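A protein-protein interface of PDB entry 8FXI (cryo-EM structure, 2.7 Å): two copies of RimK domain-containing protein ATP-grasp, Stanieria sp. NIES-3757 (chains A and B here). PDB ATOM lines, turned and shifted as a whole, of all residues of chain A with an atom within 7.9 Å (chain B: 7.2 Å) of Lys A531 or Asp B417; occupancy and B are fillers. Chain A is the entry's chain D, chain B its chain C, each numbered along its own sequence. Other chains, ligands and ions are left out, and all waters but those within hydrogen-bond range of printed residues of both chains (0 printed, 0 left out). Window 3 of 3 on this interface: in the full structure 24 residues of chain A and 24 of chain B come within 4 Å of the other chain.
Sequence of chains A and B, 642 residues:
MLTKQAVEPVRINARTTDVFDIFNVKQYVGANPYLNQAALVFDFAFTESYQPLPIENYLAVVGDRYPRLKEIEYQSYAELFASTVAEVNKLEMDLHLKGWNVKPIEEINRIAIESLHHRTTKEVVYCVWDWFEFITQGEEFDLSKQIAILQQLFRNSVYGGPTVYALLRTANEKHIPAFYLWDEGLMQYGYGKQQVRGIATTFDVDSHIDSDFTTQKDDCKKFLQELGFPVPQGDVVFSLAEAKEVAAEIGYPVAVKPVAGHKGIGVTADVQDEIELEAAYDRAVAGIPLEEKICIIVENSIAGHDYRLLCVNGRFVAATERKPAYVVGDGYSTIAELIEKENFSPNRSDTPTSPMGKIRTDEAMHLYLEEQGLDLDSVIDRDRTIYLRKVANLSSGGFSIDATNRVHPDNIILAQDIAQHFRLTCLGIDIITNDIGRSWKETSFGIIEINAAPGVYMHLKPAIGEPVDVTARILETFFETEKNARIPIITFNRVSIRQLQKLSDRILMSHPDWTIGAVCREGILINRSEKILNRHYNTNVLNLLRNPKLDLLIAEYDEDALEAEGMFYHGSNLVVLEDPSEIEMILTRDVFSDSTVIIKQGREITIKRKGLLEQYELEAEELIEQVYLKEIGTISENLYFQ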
ATOM      1  N   ALA A 518      13.332  31.121  21.692  1.00  0.00           N
ATOM      2  CA  ALA A 518      13.957  30.540  22.872  1.00  0.00           C
ATOM      3  C   ALA A 518      15.287  29.901  22.512  1.00  0.00           C
ATOM      4  O   ALA A 518      15.405  29.248  21.473  1.00  0.00           O
ATOM      5  CB  ALA A 518      13.042  29.500  23.509  1.00  0.00           C
ATOM      6  N   GLU A 522      21.081  23.212  24.393  1.00  0.00           N
ATOM      7  CA  GLU A 522      20.731  22.011  23.648  1.00  0.00           C
ATOM      8  C   GLU A 522      20.098  22.293  22.296  1.00  0.00           C
ATOM      9  O   GLU A 522      20.125  21.420  21.424  1.00  0.00           O
ATOM     10  CB  GLU A 522      19.775  21.142  24.470  1.00  0.00           C
ATOM     11  CG  GLU A 522      20.346  20.683  25.796  1.00  0.00           C
ATOM     12  CD  GLU A 522      19.435  19.713  26.521  1.00  0.00           C
ATOM     13  OE1 GLU A 522      18.290  19.517  26.069  1.00  0.00           O
ATOM     14  OE2 GLU A 522      19.864  19.141  27.545  1.00  0.00           O
ATOM     15  N   GLY A 523      19.531  23.474  22.090  1.00  0.00           N
ATOM     16  CA  GLY A 523      18.883  23.765  20.826  1.00  0.00           C
ATOM     17  C   GLY A 523      18.314  25.162  20.828  1.00  0.00           C
ATOM     18  O   GLY A 523      18.457  25.917  21.791  1.00  0.00           O
ATOM     19  N   ILE A 524      17.666  25.501  19.717  1.00  0.00           N
ATOM     20  CA  ILE A 524      17.068  26.813  19.513  1.00  0.00           C
ATOM     21  C   ILE A 524      15.699  26.625  18.874  1.00  0.00           C
ATOM     22  O   ILE A 524      15.539  25.811  17.961  1.00  0.00           O
ATOM     23  CB  ILE A 524      17.985  27.707  18.653  1.00  0.00           C
ATOM     24  CG1 ILE A 524      17.291  29.007  18.271  1.00  0.00           C
ATOM     25  CG2 ILE A 524      18.459  26.971  17.429  1.00  0.00           C
ATOM     26  CD1 ILE A 524      18.212  29.986  17.613  1.00  0.00           C
ATOM     27  N   LEU A 525      14.705  27.363  19.367  1.00  0.00           N
ATOM     28  CA  LEU A 525      13.322  27.193  18.941  1.00  0.00           C
ATOM     29  C   LEU A 525      12.707  28.524  18.544  1.00  0.00           C
ATOM     30  O   LEU A 525      12.947  29.550  19.191  1.00  0.00           O
ATOM     31  CB  LEU A 525      12.459  26.588  20.047  1.00  0.00           C
ATOM     32  CG  LEU A 525      12.733  25.200  20.600  1.00  0.00           C
ATOM     33  CD1 LEU A 525      12.293  25.170  22.036  1.00  0.00           C
ATOM     34  CD2 LEU A 525      11.975  24.168  19.815  1.00  0.00           C
ATOM     35  N   ILE A 526      11.894  28.490  17.493  1.00  0.00           N
ATOM     36  CA  ILE A 526      10.944  29.547  17.172  1.00  0.00           C
ATOM     37  C   ILE A 526       9.553  28.938  17.244  1.00  0.00           C
ATOM     38  O   ILE A 526       9.213  28.068  16.437  1.00  0.00           O
ATOM     39  CB  ILE A 526      11.199  30.163  15.791  1.00  0.00           C
ATOM     40  CG1 ILE A 526      12.502  30.958  15.799  1.00  0.00           C
ATOM     41  CG2 ILE A 526      10.050  31.058  15.398  1.00  0.00           C
ATOM     42  CD1 ILE A 526      12.729  31.755  14.553  1.00  0.00           C
ATOM     43  N   ASN A 527       8.751  29.402  18.203  1.00  0.00           N
ATOM     44  CA  ASN A 527       7.472  28.785  18.539  1.00  0.00           C
ATOM     45  C   ASN A 527       7.668  27.319  18.904  1.00  0.00           C
ATOM     46  O   ASN A 527       8.173  27.014  19.987  1.00  0.00           O
ATOM     47  CB  ASN A 527       6.467  28.941  17.397  1.00  0.00           C
ATOM     48  CG  ASN A 527       5.838  30.315  17.368  1.00  0.00           C
ATOM     49  OD1 ASN A 527       5.605  30.924  18.407  1.00  0.00           O
ATOM     50  ND2 ASN A 527       5.556  30.810  16.176  1.00  0.00           N
ATOM     51  N   ARG A 528       7.277  26.402  18.022  1.00  0.00           N
ATOM     52  CA  ARG A 528       7.370  24.975  18.302  1.00  0.00           C
ATOM     53  C   ARG A 528       8.394  24.262  17.430  1.00  0.00           C
ATOM     54  O   ARG A 528       8.593  23.056  17.592  1.00  0.00           O
ATOM     55  CB  ARG A 528       6.006  24.312  18.123  1.00  0.00           C
ATOM     56  CG  ARG A 528       4.892  24.903  18.960  1.00  0.00           C
ATOM     57  CD  ARG A 528       4.995  24.449  20.393  1.00  0.00           C
ATOM     58  NE  ARG A 528       4.992  22.997  20.509  1.00  0.00           N
ATOM     59  CZ  ARG A 528       3.932  22.271  20.834  1.00  0.00           C
ATOM     60  NH1 ARG A 528       2.755  22.831  21.065  1.00  0.00           N
ATOM     61  NH2 ARG A 528       4.054  20.952  20.934  1.00  0.00           N
ATOM     62  N   SER A 529       9.050  24.970  16.520  1.00  0.00           N
ATOM     63  CA  SER A 529       9.900  24.353  15.513  1.00  0.00           C
ATOM     64  C   SER A 529      11.369  24.437  15.906  1.00  0.00           C
ATOM     65  O   SER A 529      11.765  25.207  16.779  1.00  0.00           O
ATOM     66  CB  SER A 529       9.673  25.022  14.160  1.00  0.00           C
ATOM     67  OG  SER A 529       8.294  25.077  13.855  1.00  0.00           O
ATOM     68  N   GLU A 530      12.185  23.642  15.221  1.00  0.00           N
ATOM     69  CA  GLU A 530      13.599  23.492  15.527  1.00  0.00           C
ATOM     70  C   GLU A 530      14.451  24.134  14.442  1.00  0.00           C
ATOM     71  O   GLU A 530      14.109  24.075  13.259  1.00  0.00           O
ATOM     72  CB  GLU A 530      13.975  22.020  15.649  1.00  0.00           C
ATOM     73  CG  GLU A 530      13.241  21.286  16.737  1.00  0.00           C
ATOM     74  CD  GLU A 530      14.037  21.215  18.016  1.00  0.00           C
ATOM     75  OE1 GLU A 530      15.099  21.867  18.092  1.00  0.00           O
ATOM     76  OE2 GLU A 530      13.607  20.499  18.944  1.00  0.00           O
ATOM     77  N   LYS A 531      15.570  24.731  14.851  1.00  0.00           N
ATOM     78  CA  LYS A 531      16.498  25.360  13.919  1.00  0.00           C
ATOM     79  C   LYS A 531      17.909  24.820  14.118  1.00  0.00           C
ATOM     80  O   LYS A 531      18.103  23.830  14.826  1.00  0.00           O
ATOM     81  CB  LYS A 531      16.480  26.877  14.088  1.00  0.00           C
ATOM     82  CG  LYS A 531      15.099  27.499  14.033  1.00  0.00           C
ATOM     83  CD  LYS A 531      14.421  27.242  12.703  1.00  0.00           C
ATOM     84  CE  LYS A 531      13.011  27.798  12.683  1.00  0.00           C
ATOM     85  NZ  LYS A 531      12.296  27.468  11.425  1.00  0.00           N
ATOM     86  N   ILE A 532      18.896  25.458  13.494  1.00  0.00           N
ATOM     87  CA  ILE A 532      20.292  25.036  13.569  1.00  0.00           C
ATOM     88  C   ILE A 532      21.013  25.870  14.614  1.00  0.00           C
ATOM     89  O   ILE A 532      20.790  27.079  14.724  1.00  0.00           O
ATOM     90  CB  ILE A 532      20.970  25.159  12.194  1.00  0.00           C
ATOM     91  CG1 ILE A 532      20.152  24.435  11.132  1.00  0.00           C
ATOM     92  CG2 ILE A 532      22.363  24.584  12.235  1.00  0.00           C
ATOM     93  CD1 ILE A 532      20.093  22.950  11.328  1.00  0.00           C
ATOM     94  N   LEU A 533      21.893  25.231  15.379  1.00  0.00           N
ATOM     95  CA  LEU A 533      22.606  25.867  16.478  1.00  0.00           C
ATOM     96  C   LEU A 533      24.041  26.156  16.059  1.00  0.00           C
ATOM     97  O   LEU A 533      24.701  25.302  15.463  1.00  0.00           O
ATOM     98  CB  LEU A 533      22.583  24.975  17.718  1.00  0.00           C
ATOM     99  CG  LEU A 533      23.075  25.560  19.040  1.00  0.00           C
ATOM    100  CD1 LEU A 533      22.108  26.593  19.562  1.00  0.00           C
ATOM    101  CD2 LEU A 533      23.266  24.463  20.057  1.00  0.00           C
ATOM    102  N   ASN A 534      24.520  27.351  16.380  1.00  0.00           N
ATOM    103  CA  ASN A 534      25.843  27.803  15.983  1.00  0.00           C
ATOM    104  C   ASN A 534      26.896  27.376  17.002  1.00  0.00           C
ATOM    105  O   ASN A 534      26.598  27.093  18.162  1.00  0.00           O
ATOM    106  CB  ASN A 534      25.852  29.323  15.822  1.00  0.00           C
ATOM    107  CG  ASN A 534      26.991  29.817  14.959  1.00  0.00           C
ATOM    108  OD1 ASN A 534      28.095  29.280  15.000  1.00  0.00           O
ATOM    109  ND2 ASN A 534      26.726  30.842  14.166  1.00  0.00           N
ATOM    110  N   LEU A 544      18.653  36.068  16.998  1.00  0.00           N
ATOM    111  CA  LEU A 544      17.273  36.201  17.451  1.00  0.00           C
ATOM    112  C   LEU A 544      16.855  37.662  17.568  1.00  0.00           C
ATOM    113  O   LEU A 544      15.733  38.018  17.200  1.00  0.00           O
ATOM    114  CB  LEU A 544      17.082  35.479  18.778  1.00  0.00           C
ATOM    115  CG  LEU A 544      16.907  33.971  18.651  1.00  0.00           C
ATOM    116  CD1 LEU A 544      16.802  33.351  20.013  1.00  0.00           C
ATOM    117  CD2 LEU A 544      15.675  33.666  17.841  1.00  0.00           C
ATOM    118  N   ASN A 547      15.856  39.406  14.203  1.00  0.00           N
ATOM    119  CA  ASN A 547      14.636  38.968  13.528  1.00  0.00           C
ATOM    120  C   ASN A 547      13.586  40.074  13.533  1.00  0.00           C
ATOM    121  O   ASN A 547      13.255  40.593  14.606  1.00  0.00           O
ATOM    122  CB  ASN A 547      14.095  37.724  14.225  1.00  0.00           C
ATOM    123  CG  ASN A 547      13.110  36.956  13.380  1.00  0.00           C
ATOM    124  OD1 ASN A 547      12.262  37.532  12.710  1.00  0.00           O
ATOM    125  ND2 ASN A 547      13.213  35.639  13.414  1.00  0.00           N
ATOM    126  N   PRO A 548      13.021  40.444  12.380  1.00  0.00           N
ATOM    127  CA  PRO A 548      12.108  41.594  12.343  1.00  0.00           C
ATOM    128  C   PRO A 548      10.691  41.291  12.796  1.00  0.00           C
ATOM    129  O   PRO A 548       9.792  42.103  12.564  1.00  0.00           O
ATOM    130  CB  PRO A 548      12.119  42.002  10.864  1.00  0.00           C
ATOM    131  CG  PRO A 548      13.222  41.229  10.235  1.00  0.00           C
ATOM    132  CD  PRO A 548      13.369  39.990  11.029  1.00  0.00           C
ATOM    133  N   LEU B 227      23.632  31.449   9.500  1.00  0.00           N
ATOM    134  CA  LEU B 227      22.310  31.125  10.024  1.00  0.00           C
ATOM    135  C   LEU B 227      21.865  29.705   9.684  1.00  0.00           C
ATOM    136  O   LEU B 227      20.698  29.371   9.902  1.00  0.00           O
ATOM    137  CB  LEU B 227      21.252  32.091   9.492  1.00  0.00           C
ATOM    138  CG  LEU B 227      21.018  33.425  10.195  1.00  0.00           C
ATOM    139  CD1 LEU B 227      22.225  34.320  10.073  1.00  0.00           C
ATOM    140  CD2 LEU B 227      19.805  34.101   9.604  1.00  0.00           C
ATOM    141  N   PHE B 229      21.296  27.400   6.435  1.00  0.00           N
ATOM    142  CA  PHE B 229      21.139  27.791   5.037  1.00  0.00           C
ATOM    143  C   PHE B 229      22.256  27.266   4.143  1.00  0.00           C
ATOM    144  O   PHE B 229      23.218  27.991   3.874  1.00  0.00           O
ATOM    145  CB  PHE B 229      21.047  29.311   4.925  1.00  0.00           C
ATOM    146  CG  PHE B 229      19.848  29.895   5.607  1.00  0.00           C
ATOM    147  CD1 PHE B 229      18.824  29.087   6.055  1.00  0.00           C
ATOM    148  CD2 PHE B 229      19.743  31.255   5.798  1.00  0.00           C
ATOM    149  CE1 PHE B 229      17.730  29.623   6.684  1.00  0.00           C
ATOM    150  CE2 PHE B 229      18.648  31.795   6.426  1.00  0.00           C
ATOM    151  CZ  PHE B 229      17.641  30.978   6.869  1.00  0.00           C
ATOM    152  N   GLY B 314       6.742  37.936   1.240  1.00  0.00           N
ATOM    153  CA  GLY B 314       7.177  36.920   2.171  1.00  0.00           C
ATOM    154  C   GLY B 314       6.506  35.577   2.028  1.00  0.00           C
ATOM    155  O   GLY B 314       6.633  34.746   2.930  1.00  0.00           O
ATOM    156  N   ASP B 410       9.576  21.403   3.384  1.00  0.00           N
ATOM    157  CA  ASP B 410      10.777  21.916   4.035  1.00  0.00           C
ATOM    158  C   ASP B 410      11.411  23.033   3.220  1.00  0.00           C
ATOM    159  O   ASP B 410      11.839  24.053   3.774  1.00  0.00           O
ATOM    160  CB  ASP B 410      11.779  20.785   4.253  1.00  0.00           C
ATOM    161  CG  ASP B 410      11.334  19.815   5.321  1.00  0.00           C
ATOM    162  OD1 ASP B 410      10.207  19.966   5.830  1.00  0.00           O
ATOM    163  OD2 ASP B 410      12.117  18.904   5.657  1.00  0.00           O
ATOM    164  N   ASN B 411      11.475  22.861   1.901  1.00  0.00           N
ATOM    165  CA  ASN B 411      12.050  23.890   1.048  1.00  0.00           C
ATOM    166  C   ASN B 411      11.199  25.152   1.041  1.00  0.00           C
ATOM    167  O   ASN B 411      11.740  26.262   0.975  1.00  0.00           O
ATOM    168  CB  ASN B 411      12.230  23.341  -0.361  1.00  0.00           C
ATOM    169  CG  ASN B 411      12.964  22.021  -0.372  1.00  0.00           C
ATOM    170  OD1 ASN B 411      13.589  21.647   0.612  1.00  0.00           O
ATOM    171  ND2 ASN B 411      12.897  21.311  -1.486  1.00  0.00           N
ATOM    172  N   ILE B 412       9.877  25.008   1.124  1.00  0.00           N
ATOM    173  CA  ILE B 412       9.002  26.174   1.214  1.00  0.00           C
ATOM    174  C   ILE B 412       9.298  26.960   2.484  1.00  0.00           C
ATOM    175  O   ILE B 412       9.400  28.196   2.469  1.00  0.00           O
ATOM    176  CB  ILE B 412       7.528  25.738   1.155  1.00  0.00           C
ATOM    177  CG1 ILE B 412       7.203  25.133  -0.207  1.00  0.00           C
ATOM    178  CG2 ILE B 412       6.617  26.902   1.450  1.00  0.00           C
ATOM    179  CD1 ILE B 412       5.781  24.679  -0.336  1.00  0.00           C
ATOM    180  N   ILE B 413       9.444  26.254   3.604  1.00  0.00           N
ATOM    181  CA  ILE B 413       9.736  26.935   4.861  1.00  0.00           C
ATOM    182  C   ILE B 413      11.105  27.603   4.806  1.00  0.00           C
ATOM    183  O   ILE B 413      11.292  28.709   5.329  1.00  0.00           O
ATOM    184  CB  ILE B 413       9.624  25.947   6.031  1.00  0.00           C
ATOM    185  CG1 ILE B 413       8.205  25.387   6.093  1.00  0.00           C
ATOM    186  CG2 ILE B 413       9.980  26.623   7.330  1.00  0.00           C
ATOM    187  CD1 ILE B 413       7.978  24.427   7.210  1.00  0.00           C
ATOM    188  N   LEU B 414      12.076  26.953   4.167  1.00  0.00           N
ATOM    189  CA  LEU B 414      13.391  27.565   4.002  1.00  0.00           C
ATOM    190  C   LEU B 414      13.306  28.861   3.204  1.00  0.00           C
ATOM    191  O   LEU B 414      13.932  29.869   3.564  1.00  0.00           O
ATOM    192  CB  LEU B 414      14.331  26.575   3.318  1.00  0.00           C
ATOM    193  CG  LEU B 414      15.744  27.040   2.989  1.00  0.00           C
ATOM    194  CD1 LEU B 414      16.534  27.219   4.255  1.00  0.00           C
ATOM    195  CD2 LEU B 414      16.419  26.041   2.088  1.00  0.00           C
ATOM    196  N   ALA B 415      12.536  28.854   2.117  1.00  0.00           N
ATOM    197  CA  ALA B 415      12.389  30.058   1.307  1.00  0.00           C
ATOM    198  C   ALA B 415      11.731  31.182   2.095  1.00  0.00           C
ATOM    199  O   ALA B 415      12.152  32.340   2.004  1.00  0.00           O
ATOM    200  CB  ALA B 415      11.587  29.749   0.048  1.00  0.00           C
ATOM    201  N   GLN B 416      10.696  30.863   2.875  1.00  0.00           N
ATOM    202  CA  GLN B 416      10.064  31.890   3.700  1.00  0.00           C
ATOM    203  C   GLN B 416      11.048  32.477   4.704  1.00  0.00           C
ATOM    204  O   GLN B 416      11.079  33.697   4.922  1.00  0.00           O
ATOM    205  CB  GLN B 416       8.857  31.315   4.432  1.00  0.00           C
ATOM    206  CG  GLN B 416       7.734  30.870   3.540  1.00  0.00           C
ATOM    207  CD  GLN B 416       6.593  30.270   4.320  1.00  0.00           C
ATOM    208  OE1 GLN B 416       5.580  29.874   3.753  1.00  0.00           O
ATOM    209  NE2 GLN B 416       6.751  30.196   5.630  1.00  0.00           N
ATOM    210  N   ASP B 417      11.853  31.617   5.334  1.00  0.00           N
ATOM    211  CA  ASP B 417      12.830  32.092   6.307  1.00  0.00           C
ATOM    212  C   ASP B 417      13.838  33.033   5.668  1.00  0.00           C
ATOM    213  O   ASP B 417      14.207  34.051   6.262  1.00  0.00           O
ATOM    214  CB  ASP B 417      13.551  30.914   6.952  1.00  0.00           C
ATOM    215  CG  ASP B 417      12.635  30.063   7.797  1.00  0.00           C
ATOM    216  OD1 ASP B 417      11.419  30.344   7.828  1.00  0.00           O
ATOM    217  OD2 ASP B 417      13.132  29.109   8.433  1.00  0.00           O
ATOM    218  N   ILE B 418      14.316  32.701   4.470  1.00  0.00           N
ATOM    219  CA  ILE B 418      15.244  33.601   3.789  1.00  0.00           C
ATOM    220  C   ILE B 418      14.563  34.922   3.463  1.00  0.00           C
ATOM    221  O   ILE B 418      15.121  36.001   3.687  1.00  0.00           O
ATOM    222  CB  ILE B 418      15.814  32.945   2.521  1.00  0.00           C
ATOM    223  CG1 ILE B 418      16.688  31.752   2.875  1.00  0.00           C
ATOM    224  CG2 ILE B 418      16.618  33.948   1.735  1.00  0.00           C
ATOM    225  CD1 ILE B 418      17.313  31.110   1.680  1.00  0.00           C
ATOM    226  N   ALA B 419      13.340  34.861   2.937  1.00  0.00           N
ATOM    227  CA  ALA B 419      12.698  36.062   2.418  1.00  0.00           C
ATOM    228  C   ALA B 419      12.258  37.027   3.506  1.00  0.00           C
ATOM    229  O   ALA B 419      12.099  38.216   3.224  1.00  0.00           O
ATOM    230  CB  ALA B 419      11.492  35.688   1.563  1.00  0.00           C
ATOM    231  N   GLN B 420      12.048  36.558   4.731  1.00  0.00           N
ATOM    232  CA  GLN B 420      11.516  37.492   5.721  1.00  0.00           C
ATOM    233  C   GLN B 420      12.539  38.501   6.238  1.00  0.00           C
ATOM    234  O   GLN B 420      12.159  39.359   7.037  1.00  0.00           O
ATOM    235  CB  GLN B 420      10.931  36.733   6.906  1.00  0.00           C
ATOM    236  CG  GLN B 420      11.965  36.242   7.885  1.00  0.00           C
ATOM    237  CD  GLN B 420      11.348  35.553   9.072  1.00  0.00           C
ATOM    238  OE1 GLN B 420      10.155  35.685   9.326  1.00  0.00           O
ATOM    239  NE2 GLN B 420      12.157  34.806   9.807  1.00  0.00           N
ATOM    240  N   HIS B 421      13.804  38.437   5.832  1.00  0.00           N
ATOM    241  CA  HIS B 421      14.837  39.298   6.396  1.00  0.00           C
ATOM    242  C   HIS B 421      15.078  40.582   5.611  1.00  0.00           C
ATOM    243  O   HIS B 421      15.924  41.381   6.019  1.00  0.00           O
ATOM    244  CB  HIS B 421      16.160  38.535   6.507  1.00  0.00           C
ATOM    245  CG  HIS B 421      16.248  37.647   7.707  1.00  0.00           C
ATOM    246  ND1 HIS B 421      16.674  38.099   8.936  1.00  0.00           N
ATOM    247  CD2 HIS B 421      15.966  36.334   7.868  1.00  0.00           C
ATOM    248  CE1 HIS B 421      16.647  37.104   9.802  1.00  0.00           C
ATOM    249  NE2 HIS B 421      16.220  36.022   9.179  1.00  0.00           N
ATOM    250  N   PHE B 422      14.370  40.812   4.510  1.00  0.00           N
ATOM    251  CA  PHE B 422      14.605  41.968   3.657  1.00  0.00           C
ATOM    252  C   PHE B 422      13.331  42.784   3.499  1.00  0.00           C
ATOM    253  O   PHE B 422      12.223  42.256   3.593  1.00  0.00           O
ATOM    254  CB  PHE B 422      15.103  41.547   2.276  1.00  0.00           C
ATOM    255  CG  PHE B 422      16.349  40.723   2.301  1.00  0.00           C
ATOM    256  CD1 PHE B 422      17.584  41.316   2.463  1.00  0.00           C
ATOM    257  CD2 PHE B 422      16.290  39.354   2.143  1.00  0.00           C
ATOM    258  CE1 PHE B 422      18.731  40.558   2.478  1.00  0.00           C
ATOM    259  CE2 PHE B 422      17.436  38.593   2.158  1.00  0.00           C
ATOM    260  CZ  PHE B 422      18.656  39.195   2.324  1.00  0.00           C
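Along chain B the printed residues that touch a printed residue of chain A span positions 417 to 420.
Among the printed residues, Asp or Glu carboxylates within 4 Å of a Lys or Arg side-chain nitrogen of the other chain: Lys A531 with Asp B417 (3.5 Å).
No position is printed for both chains.
Of the 3 pairs that touch across the chains among the printed residues, none has its exchanged pair printed and touching as well.
The side-chain amino group (NZ) of Lys A531 is in salt-bridge range of the side-chain carboxylate (OD2) of Asp B417 (3.5 Å).
Among the printed residues, merely in contact across the chains: Asn A547 with Gln B420 (3.8 Å) and Pro A548 with Gln B420 (3.9 Å).
The backbone carbonyl oxygen of Ile A524 lies within hydrogen-bond range of the backbone NH of Lys A531 (3.3 Å).
Lys A531 touches just one residue of chain B: Asp B417 (3.5 Å).
Of the printed residues of chain B, Pro A548 touches Gln B420 (3.9 Å).
Of the printed residues of chain A, Gln B420 touches Asn A547 and Pro A548.
Of the printed residues of chain B, Asn A547 touches Gln B420.
The nearest residue of chain A that does not touch Asp B417 is Ile A526 (6.7 Å).
The nearest printed residue of chain A that does not touch Gln B420 is Ile A526 (5.7 Å).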
